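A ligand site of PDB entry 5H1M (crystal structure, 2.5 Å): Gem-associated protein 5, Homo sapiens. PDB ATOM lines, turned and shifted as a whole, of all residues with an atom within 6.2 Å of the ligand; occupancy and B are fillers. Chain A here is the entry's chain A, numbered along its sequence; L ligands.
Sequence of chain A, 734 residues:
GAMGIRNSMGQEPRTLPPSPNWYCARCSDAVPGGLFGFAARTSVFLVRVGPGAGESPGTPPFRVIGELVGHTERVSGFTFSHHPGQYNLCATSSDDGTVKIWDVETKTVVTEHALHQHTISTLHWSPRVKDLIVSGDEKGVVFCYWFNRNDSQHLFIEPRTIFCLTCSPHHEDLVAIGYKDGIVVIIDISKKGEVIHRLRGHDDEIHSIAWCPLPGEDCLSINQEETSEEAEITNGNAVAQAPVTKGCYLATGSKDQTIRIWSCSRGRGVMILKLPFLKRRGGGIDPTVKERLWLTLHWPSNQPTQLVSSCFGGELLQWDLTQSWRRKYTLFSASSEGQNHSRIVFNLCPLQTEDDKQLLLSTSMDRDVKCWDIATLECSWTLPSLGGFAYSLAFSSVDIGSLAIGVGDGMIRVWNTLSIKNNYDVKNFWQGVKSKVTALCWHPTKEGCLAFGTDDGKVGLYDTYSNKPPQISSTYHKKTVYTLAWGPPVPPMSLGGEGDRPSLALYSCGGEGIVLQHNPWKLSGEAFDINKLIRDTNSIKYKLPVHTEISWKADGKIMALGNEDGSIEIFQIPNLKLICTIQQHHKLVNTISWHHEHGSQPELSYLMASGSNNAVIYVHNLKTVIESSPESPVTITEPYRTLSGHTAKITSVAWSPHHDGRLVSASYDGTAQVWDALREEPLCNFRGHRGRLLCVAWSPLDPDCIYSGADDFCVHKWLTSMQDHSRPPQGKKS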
ATOM      1  N   TYR A 391     -23.912 -27.648 -28.510  1.00  0.00           N
ATOM      2  CA  TYR A 391     -24.415 -27.573 -27.145  1.00  0.00           C
ATOM      3  C   TYR A 391     -23.782 -28.580 -26.189  1.00  0.00           C
ATOM      4  O   TYR A 391     -23.369 -28.211 -25.088  1.00  0.00           O
ATOM      5  CB  TYR A 391     -25.933 -27.763 -27.121  1.00  0.00           C
ATOM      6  CG  TYR A 391     -26.736 -26.613 -27.693  1.00  0.00           C
ATOM      7  CD1 TYR A 391     -26.983 -25.471 -26.936  1.00  0.00           C
ATOM      8  CD2 TYR A 391     -27.273 -26.675 -28.975  1.00  0.00           C
ATOM      9  CE1 TYR A 391     -27.720 -24.422 -27.443  1.00  0.00           C
ATOM     10  CE2 TYR A 391     -28.019 -25.632 -29.491  1.00  0.00           C
ATOM     11  CZ  TYR A 391     -28.234 -24.504 -28.723  1.00  0.00           C
ATOM     12  OH  TYR A 391     -28.980 -23.461 -29.240  1.00  0.00           O
ATOM     13  N   THR A 480     -36.246 -26.050 -22.096  1.00  0.00           N
ATOM     14  CA  THR A 480     -35.106 -26.747 -22.661  1.00  0.00           C
ATOM     15  C   THR A 480     -34.512 -27.800 -21.725  1.00  0.00           C
ATOM     16  O   THR A 480     -34.256 -27.516 -20.554  1.00  0.00           O
ATOM     17  CB  THR A 480     -33.992 -25.744 -23.059  1.00  0.00           C
ATOM     18  OG1 THR A 480     -34.434 -24.965 -24.167  1.00  0.00           O
ATOM     19  CG2 THR A 480     -32.707 -26.476 -23.429  1.00  0.00           C
ATOM     20  N   TYR A 482     -31.600 -29.371 -20.291  1.00  0.00           N
ATOM     21  CA  TYR A 482     -30.203 -28.930 -20.148  1.00  0.00           C
ATOM     22  C   TYR A 482     -29.298 -30.046 -19.669  1.00  0.00           C
ATOM     23  O   TYR A 482     -28.082 -29.969 -19.833  1.00  0.00           O
ATOM     24  CB  TYR A 482     -30.115 -27.744 -19.189  1.00  0.00           C
ATOM     25  CG  TYR A 482     -30.590 -26.430 -19.783  1.00  0.00           C
ATOM     26  CD1 TYR A 482     -29.828 -25.768 -20.733  1.00  0.00           C
ATOM     27  CD2 TYR A 482     -31.789 -25.863 -19.389  1.00  0.00           C
ATOM     28  CE1 TYR A 482     -30.257 -24.577 -21.283  1.00  0.00           C
ATOM     29  CE2 TYR A 482     -32.227 -24.670 -19.933  1.00  0.00           C
ATOM     30  CZ  TYR A 482     -31.453 -24.036 -20.877  1.00  0.00           C
ATOM     31  OH  TYR A 482     -31.887 -22.833 -21.419  1.00  0.00           O
ATOM     32  N   THR A 483     -29.871 -31.082 -19.063  1.00  0.00           N
ATOM     33  CA  THR A 483     -29.056 -32.140 -18.485  1.00  0.00           C
ATOM     34  C   THR A 483     -29.737 -33.499 -18.551  1.00  0.00           C
ATOM     35  O   THR A 483     -30.945 -33.620 -18.348  1.00  0.00           O
ATOM     36  CB  THR A 483     -28.724 -31.832 -17.008  1.00  0.00           C
ATOM     37  OG1 THR A 483     -28.387 -30.447 -16.864  1.00  0.00           O
ATOM     38  CG2 THR A 483     -27.550 -32.700 -16.539  1.00  0.00           C
ATOM     39  N   CYS A 509     -33.312 -33.027 -16.633  1.00  0.00           N
ATOM     40  CA  CYS A 509     -33.589 -31.759 -15.968  1.00  0.00           C
ATOM     41  C   CYS A 509     -33.907 -30.682 -17.004  1.00  0.00           C
ATOM     42  O   CYS A 509     -33.160 -30.488 -17.968  1.00  0.00           O
ATOM     43  CB  CYS A 509     -32.397 -31.343 -15.105  1.00  0.00           C
ATOM     44  SG  CYS A 509     -32.646 -29.778 -14.227  1.00  0.00           S
ATOM     45  N   GLY A 510     -35.012 -29.976 -16.793  1.00  0.00           N
ATOM     46  CA  GLY A 510     -35.459 -28.956 -17.728  1.00  0.00           C
ATOM     47  C   GLY A 510     -35.325 -27.553 -17.155  1.00  0.00           C
ATOM     48  O   GLY A 510     -35.170 -27.378 -15.949  1.00  0.00           O
ATOM     49  N   GLY A 511     -35.408 -26.560 -18.028  1.00  0.00           N
ATOM     50  CA  GLY A 511     -35.252 -25.163 -17.640  1.00  0.00           C
ATOM     51  C   GLY A 511     -36.269 -24.682 -16.622  1.00  0.00           C
ATOM     52  O   GLY A 511     -36.058 -23.672 -15.952  1.00  0.00           O
ATOM     53  N   HIS A 547     -34.539 -26.718 -10.009  1.00  0.00           N
ATOM     54  CA  HIS A 547     -33.331 -27.487 -10.318  1.00  0.00           C
ATOM     55  C   HIS A 547     -32.804 -27.144 -11.709  1.00  0.00           C
ATOM     56  O   HIS A 547     -33.568 -27.052 -12.666  1.00  0.00           O
ATOM     57  CB  HIS A 547     -33.603 -28.982 -10.232  1.00  0.00           C
ATOM     58  CG  HIS A 547     -34.170 -29.416  -8.917  1.00  0.00           C
ATOM     59  ND1 HIS A 547     -33.586 -29.099  -7.698  1.00  0.00           N
ATOM     60  CD2 HIS A 547     -35.270 -30.158  -8.609  1.00  0.00           C
ATOM     61  CE1 HIS A 547     -34.293 -29.613  -6.721  1.00  0.00           C
ATOM     62  NE2 HIS A 547     -35.323 -30.261  -7.242  1.00  0.00           N
ATOM     63  N   THR A 548     -31.493 -26.961 -11.814  1.00  0.00           N
ATOM     64  CA  THR A 548     -30.888 -26.572 -13.084  1.00  0.00           C
ATOM     65  C   THR A 548     -29.765 -27.502 -13.522  1.00  0.00           C
ATOM     66  O   THR A 548     -29.188 -27.333 -14.599  1.00  0.00           O
ATOM     67  CB  THR A 548     -30.346 -25.139 -13.020  1.00  0.00           C
ATOM     68  OG1 THR A 548     -29.442 -25.019 -11.911  1.00  0.00           O
ATOM     69  CG2 THR A 548     -31.476 -24.144 -12.859  1.00  0.00           C
ATOM     70  N   GLU A 549     -29.451 -28.507 -12.695  1.00  0.00           N
ATOM     71  CA  GLU A 549     -28.365 -29.426 -13.000  1.00  0.00           C
ATOM     72  C   GLU A 549     -28.458 -30.703 -12.170  1.00  0.00           C
ATOM     73  O   GLU A 549     -28.805 -30.663 -10.990  1.00  0.00           O
ATOM     74  CB  GLU A 549     -27.015 -28.738 -12.756  1.00  0.00           C
ATOM     75  CG  GLU A 549     -25.796 -29.652 -12.827  1.00  0.00           C
ATOM     76  CD  GLU A 549     -25.453 -30.091 -14.243  1.00  0.00           C
ATOM     77  OE1 GLU A 549     -26.167 -29.695 -15.191  1.00  0.00           O
ATOM     78  OE2 GLU A 549     -24.457 -30.828 -14.419  1.00  0.00           O
ATOM     79  N   LEU A 588     -27.233 -19.107 -10.845  1.00  0.00           N
ATOM     80  CA  LEU A 588     -27.702 -20.373 -11.426  1.00  0.00           C
ATOM     81  C   LEU A 588     -26.591 -21.394 -11.702  1.00  0.00           C
ATOM     82  O   LEU A 588     -25.628 -21.099 -12.421  1.00  0.00           O
ATOM     83  CB  LEU A 588     -28.487 -20.094 -12.712  1.00  0.00           C
ATOM     84  CG  LEU A 588     -29.260 -21.245 -13.370  1.00  0.00           C
ATOM     85  CD1 LEU A 588     -30.567 -20.731 -13.941  1.00  0.00           C
ATOM     86  CD2 LEU A 588     -28.439 -21.912 -14.452  1.00  0.00           C
ATOM     87  N   VAL A 589     -26.738 -22.590 -11.147  1.00  0.00           N
ATOM     88  CA  VAL A 589     -25.757 -23.663 -11.345  1.00  0.00           C
ATOM     89  C   VAL A 589     -25.904 -24.285 -12.725  1.00  0.00           C
ATOM     90  O   VAL A 589     -26.965 -24.801 -13.077  1.00  0.00           O
ATOM     91  CB  VAL A 589     -25.892 -24.752 -10.275  1.00  0.00           C
ATOM     92  CG1 VAL A 589     -24.929 -25.901 -10.557  1.00  0.00           C
ATOM     93  CG2 VAL A 589     -25.656 -24.176  -8.885  1.00  0.00           C
ATOM     94  N   ASN A 590     -24.816 -24.252 -13.502  1.00  0.00           N
ATOM     95  CA  ASN A 590     -24.840 -24.735 -14.880  1.00  0.00           C
ATOM     96  C   ASN A 590     -24.308 -26.158 -15.040  1.00  0.00           C
ATOM     97  O   ASN A 590     -24.774 -26.909 -15.899  1.00  0.00           O
ATOM     98  CB  ASN A 590     -24.027 -23.811 -15.775  1.00  0.00           C
ATOM     99  CG  ASN A 590     -24.693 -22.457 -15.965  1.00  0.00           C
ATOM    100  OD1 ASN A 590     -25.862 -22.379 -16.332  1.00  0.00           O
ATOM    101  ND2 ASN A 590     -23.934 -21.400 -15.712  1.00  0.00           N
ATOM    102  N   THR A 591     -23.334 -26.520 -14.214  1.00  0.00           N
ATOM    103  CA  THR A 591     -22.613 -27.767 -14.414  1.00  0.00           C
ATOM    104  C   THR A 591     -22.041 -28.307 -13.110  1.00  0.00           C
ATOM    105  O   THR A 591     -21.588 -27.551 -12.252  1.00  0.00           O
ATOM    106  CB  THR A 591     -21.479 -27.587 -15.441  1.00  0.00           C
ATOM    107  OG1 THR A 591     -20.629 -28.747 -15.433  1.00  0.00           O
ATOM    108  CG2 THR A 591     -20.646 -26.355 -15.110  1.00  0.00           C
ATOM    109  N   ASN A 613     -23.250 -19.070 -13.115  1.00  0.00           N
ATOM    110  CA  ASN A 613     -23.233 -17.858 -13.908  1.00  0.00           C
ATOM    111  C   ASN A 613     -22.146 -16.887 -13.440  1.00  0.00           C
ATOM    112  O   ASN A 613     -21.827 -15.924 -14.136  1.00  0.00           O
ATOM    113  CB  ASN A 613     -24.600 -17.182 -13.892  1.00  0.00           C
ATOM    114  CG  ASN A 613     -25.602 -17.875 -14.812  1.00  0.00           C
ATOM    115  OD1 ASN A 613     -25.217 -18.542 -15.776  1.00  0.00           O
ATOM    116  ND2 ASN A 613     -26.881 -17.716 -14.515  1.00  0.00           N
ATOM    117  N   LYS A 649     -19.590 -16.501 -17.312  1.00  0.00           N
ATOM    118  CA  LYS A 649     -20.263 -17.674 -16.762  1.00  0.00           C
ATOM    119  C   LYS A 649     -19.618 -18.986 -17.221  1.00  0.00           C
ATOM    120  O   LYS A 649     -19.085 -19.076 -18.330  1.00  0.00           O
ATOM    121  CB  LYS A 649     -21.751 -17.663 -17.120  1.00  0.00           C
ATOM    122  CG  LYS A 649     -22.057 -17.730 -18.601  1.00  0.00           C
ATOM    123  CD  LYS A 649     -23.541 -17.487 -18.874  1.00  0.00           C
ATOM    124  CE  LYS A 649     -23.961 -16.073 -18.485  1.00  0.00           C
ATOM    125  NZ  LYS A 649     -25.393 -15.795 -18.816  1.00  0.00           N
ATOM    126  N   THR A 651     -20.079 -22.749 -18.306  1.00  0.00           N
ATOM    127  CA  THR A 651     -21.112 -23.601 -18.888  1.00  0.00           C
ATOM    128  C   THR A 651     -20.863 -25.087 -18.665  1.00  0.00           C
ATOM    129  O   THR A 651     -21.811 -25.881 -18.676  1.00  0.00           O
ATOM    130  CB  THR A 651     -21.242 -23.349 -20.400  1.00  0.00           C
ATOM    131  OG1 THR A 651     -19.990 -23.610 -21.031  1.00  0.00           O
ATOM    132  CG2 THR A 651     -21.657 -21.912 -20.673  1.00  0.00           C
ATOM    133  N   SER A 652     -19.606 -25.468 -18.478  1.00  0.00           N
ATOM    134  CA  SER A 652     -19.253 -26.878 -18.408  1.00  0.00           C
ATOM    135  C   SER A 652     -17.887 -27.137 -17.753  1.00  0.00           C
ATOM    136  O   SER A 652     -16.913 -26.438 -18.046  1.00  0.00           O
ATOM    137  CB  SER A 652     -19.281 -27.483 -19.823  1.00  0.00           C
ATOM    138  OG  SER A 652     -18.984 -28.861 -19.817  1.00  0.00           O
ATOM    139  N   TYR A 668     -18.134 -18.554 -21.012  1.00  0.00           N
ATOM    140  CA  TYR A 668     -18.688 -17.571 -21.942  1.00  0.00           C
ATOM    141  C   TYR A 668     -17.655 -16.519 -22.327  1.00  0.00           C
ATOM    142  O   TYR A 668     -17.907 -15.682 -23.191  1.00  0.00           O
ATOM    143  CB  TYR A 668     -19.908 -16.886 -21.327  1.00  0.00           C
ATOM    144  CG  TYR A 668     -21.230 -17.341 -21.900  1.00  0.00           C
ATOM    145  CD1 TYR A 668     -21.461 -18.670 -22.207  1.00  0.00           C
ATOM    146  CD2 TYR A 668     -22.260 -16.433 -22.114  1.00  0.00           C
ATOM    147  CE1 TYR A 668     -22.669 -19.090 -22.726  1.00  0.00           C
ATOM    148  CE2 TYR A 668     -23.481 -16.848 -22.634  1.00  0.00           C
ATOM    149  CZ  TYR A 668     -23.679 -18.169 -22.935  1.00  0.00           C
ATOM    150  OH  TYR A 668     -24.884 -18.580 -23.452  1.00  0.00           O
ATOM    151  N   ARG A 692     -18.852 -18.245 -27.576  1.00  0.00           N
ATOM    152  CA  ARG A 692     -18.916 -18.612 -26.163  1.00  0.00           C
ATOM    153  C   ARG A 692     -19.099 -20.124 -25.992  1.00  0.00           C
ATOM    154  O   ARG A 692     -20.044 -20.715 -26.520  1.00  0.00           O
ATOM    155  CB  ARG A 692     -20.059 -17.848 -25.489  1.00  0.00           C
ATOM    156  CG  ARG A 692     -19.959 -16.350 -25.713  1.00  0.00           C
ATOM    157  CD  ARG A 692     -21.257 -15.648 -25.385  1.00  0.00           C
ATOM    158  NE  ARG A 692     -22.352 -16.090 -26.248  1.00  0.00           N
ATOM    159  CZ  ARG A 692     -23.596 -15.623 -26.162  1.00  0.00           C
ATOM    160  NH1 ARG A 692     -23.903 -14.689 -25.275  1.00  0.00           N
ATOM    161  NH2 ARG A 692     -24.530 -16.090 -26.978  1.00  0.00           N
ATOM    162  N   LEU A 693     -18.184 -20.740 -25.250  1.00  0.00           N
ATOM    163  CA  LEU A 693     -18.149 -22.196 -25.113  1.00  0.00           C
ATOM    164  C   LEU A 693     -19.345 -22.732 -24.327  1.00  0.00           C
ATOM    165  O   LEU A 693     -19.747 -22.165 -23.305  1.00  0.00           O
ATOM    166  CB  LEU A 693     -16.843 -22.641 -24.447  1.00  0.00           C
ATOM    167  CG  LEU A 693     -15.650 -22.733 -25.401  1.00  0.00           C
ATOM    168  CD1 LEU A 693     -15.098 -21.357 -25.755  1.00  0.00           C
ATOM    169  CD2 LEU A 693     -14.559 -23.621 -24.834  1.00  0.00           C
ATOM    170  N   LEU A 694     -19.904 -23.829 -24.824  1.00  0.00           N
ATOM    171  CA  LEU A 694     -21.107 -24.418 -24.263  1.00  0.00           C
ATOM    172  C   LEU A 694     -20.827 -25.792 -23.653  1.00  0.00           C
ATOM    173  O   LEU A 694     -21.586 -26.271 -22.818  1.00  0.00           O
ATOM    174  CB  LEU A 694     -22.178 -24.545 -25.352  1.00  0.00           C
ATOM    175  CG  LEU A 694     -22.624 -23.233 -25.993  1.00  0.00           C
ATOM    176  CD1 LEU A 694     -23.504 -23.483 -27.214  1.00  0.00           C
ATOM    177  CD2 LEU A 694     -23.358 -22.382 -24.967  1.00  0.00           C
HETATM  178  P1  LIG L   1     -29.508 -19.422 -22.333  1.00  0.00           P
HETATM  179  O1  LIG L   1     -30.315 -20.401 -23.150  1.00  0.00           O
HETATM  180  O2  LIG L   1     -30.332 -18.958 -21.145  1.00  0.00           O
HETATM  181  O3  LIG L   1     -29.154 -18.172 -23.249  1.00  0.00           O
HETATM  182  O4  LIG L   1     -28.195 -20.154 -21.823  1.00  0.00           O
HETATM  183  P2  LIG L   1     -28.086 -17.151 -22.656  1.00  0.00           P
HETATM  184  O5  LIG L   1     -28.768 -15.835 -22.376  1.00  0.00           O
HETATM  185  O6  LIG L   1     -27.023 -16.906 -23.709  1.00  0.00           O
HETATM  186  O7  LIG L   1     -27.439 -17.647 -21.384  1.00  0.00           O
HETATM  187  C1  LIG L   1     -27.599 -20.959 -22.824  1.00  0.00           C
HETATM  188  C2  LIG L   1     -26.485 -21.776 -22.215  1.00  0.00           C
HETATM  189  O8  LIG L   1     -26.371 -21.530 -20.784  1.00  0.00           O
HETATM  190  C3  LIG L   1     -26.813 -23.260 -22.370  1.00  0.00           C
HETATM  191  O9  LIG L   1     -26.140 -23.818 -23.509  1.00  0.00           O
HETATM  192  C4  LIG L   1     -26.311 -23.901 -21.076  1.00  0.00           C
HETATM  193  O10 LIG L   1     -24.949 -24.317 -21.207  1.00  0.00           O
HETATM  194  C5  LIG L   1     -26.426 -22.768 -20.066  1.00  0.00           C
HETATM  195  N1  LIG L   1     -27.670 -22.856 -19.322  1.00  0.00           N
HETATM  196  C6  LIG L   1     -28.793 -21.920 -19.384  1.00  0.00           C
HETATM  197  N2  LIG L   1     -29.812 -22.427 -18.462  1.00  0.00           N
HETATM  198  C7  LIG L   1     -31.092 -21.817 -18.199  1.00  0.00           C
HETATM  199  C8  LIG L   1     -29.309 -23.569 -17.914  1.00  0.00           C
HETATM  200  C9  LIG L   1     -29.835 -24.469 -16.972  1.00  0.00           C
HETATM  201  O11 LIG L   1     -30.935 -24.315 -16.478  1.00  0.00           O
HETATM  202  N3  LIG L   1     -29.080 -25.554 -16.596  1.00  0.00           N
HETATM  203  C10 LIG L   1     -27.862 -25.768 -17.120  1.00  0.00           C
HETATM  204  N4  LIG L   1     -27.149 -26.853 -16.715  1.00  0.00           N
HETATM  205  N5  LIG L   1     -27.328 -24.911 -18.022  1.00  0.00           N
HETATM  206  C11 LIG L   1     -28.022 -23.820 -18.436  1.00  0.00           C
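A nitrogen (N4) of the ligand sits at hydrogen-bond distance from the side-chain carboxylate (OE1) of Glu 549 (3.4 Å).
A nitrogen (N4) of the ligand is in hydrogen-bond range of the backbone carbonyl oxygen (O) of Asn 590 (2.5 Å).
An oxygen (O1) of the ligand lies within hydrogen-bond range of the side-chain hydroxyl of Tyr 482 (3.4 Å).
An oxygen (O6) of the ligand is in hydrogen-bond range of the side-chain hydroxyl (OH) of Tyr 668, at 2.7 Å.
O7 of the ligand is in salt-bridge range of NZ of Lys 649 (3.8 Å).
The backbone carbonyl oxygen (O) of Thr 548 is in hydrogen-bond range of a nitrogen (N3) of the ligand, 2.7 Å away.
N5 of the ligand sits close to OD1 of Asn 590, 3.4 Å away.
The backbone carbonyl oxygen (O) of Leu 588 is in hydrogen-bond range of the backbone NH (N) of Asn 613 (3.2 Å).
The side-chain sulfur of Cys 509 is in hydrogen-bond range of the backbone NH of Glu 549, at 3.8 Å.
The side-chain amide nitrogen (ND2) of Asn 590 lies within hydrogen-bond range of the side-chain amide oxygen (OD1) of Asn 613 (3.1 Å).
The backbone carbonyl oxygen (O) of Lys 649 is in hydrogen-bond range of the backbone NH (N) of Tyr 668, at 2.9 Å.
N of Tyr 482 is in hydrogen-bond range of O of Cys 509 (3.0 Å).
The backbone carbonyl oxygen of Val 589 lies within hydrogen-bond range of the side-chain hydroxyl of Thr 548, at 2.7 Å.
The side-chain hydroxyl (OG1) of Thr 651 lies within hydrogen-bond range of the backbone carbonyl oxygen (O) of Leu 693, at 2.7 Å.
OE1 of Glu 549 lies within hydrogen-bond range of OG1 of Thr 483 (2.9 Å).
Residues that only touch the ligand: Leu 694, Thr 483, Leu 588, Tyr 391 and Thr 651.
Hydrophobic or aromatic side chains within 4 Å of the ligand: Tyr 391, Tyr 482, Leu 588, Tyr 668 and Leu 694.
The nearest printed residue that does not touch the ligand is Arg 692 (4.1 Å).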
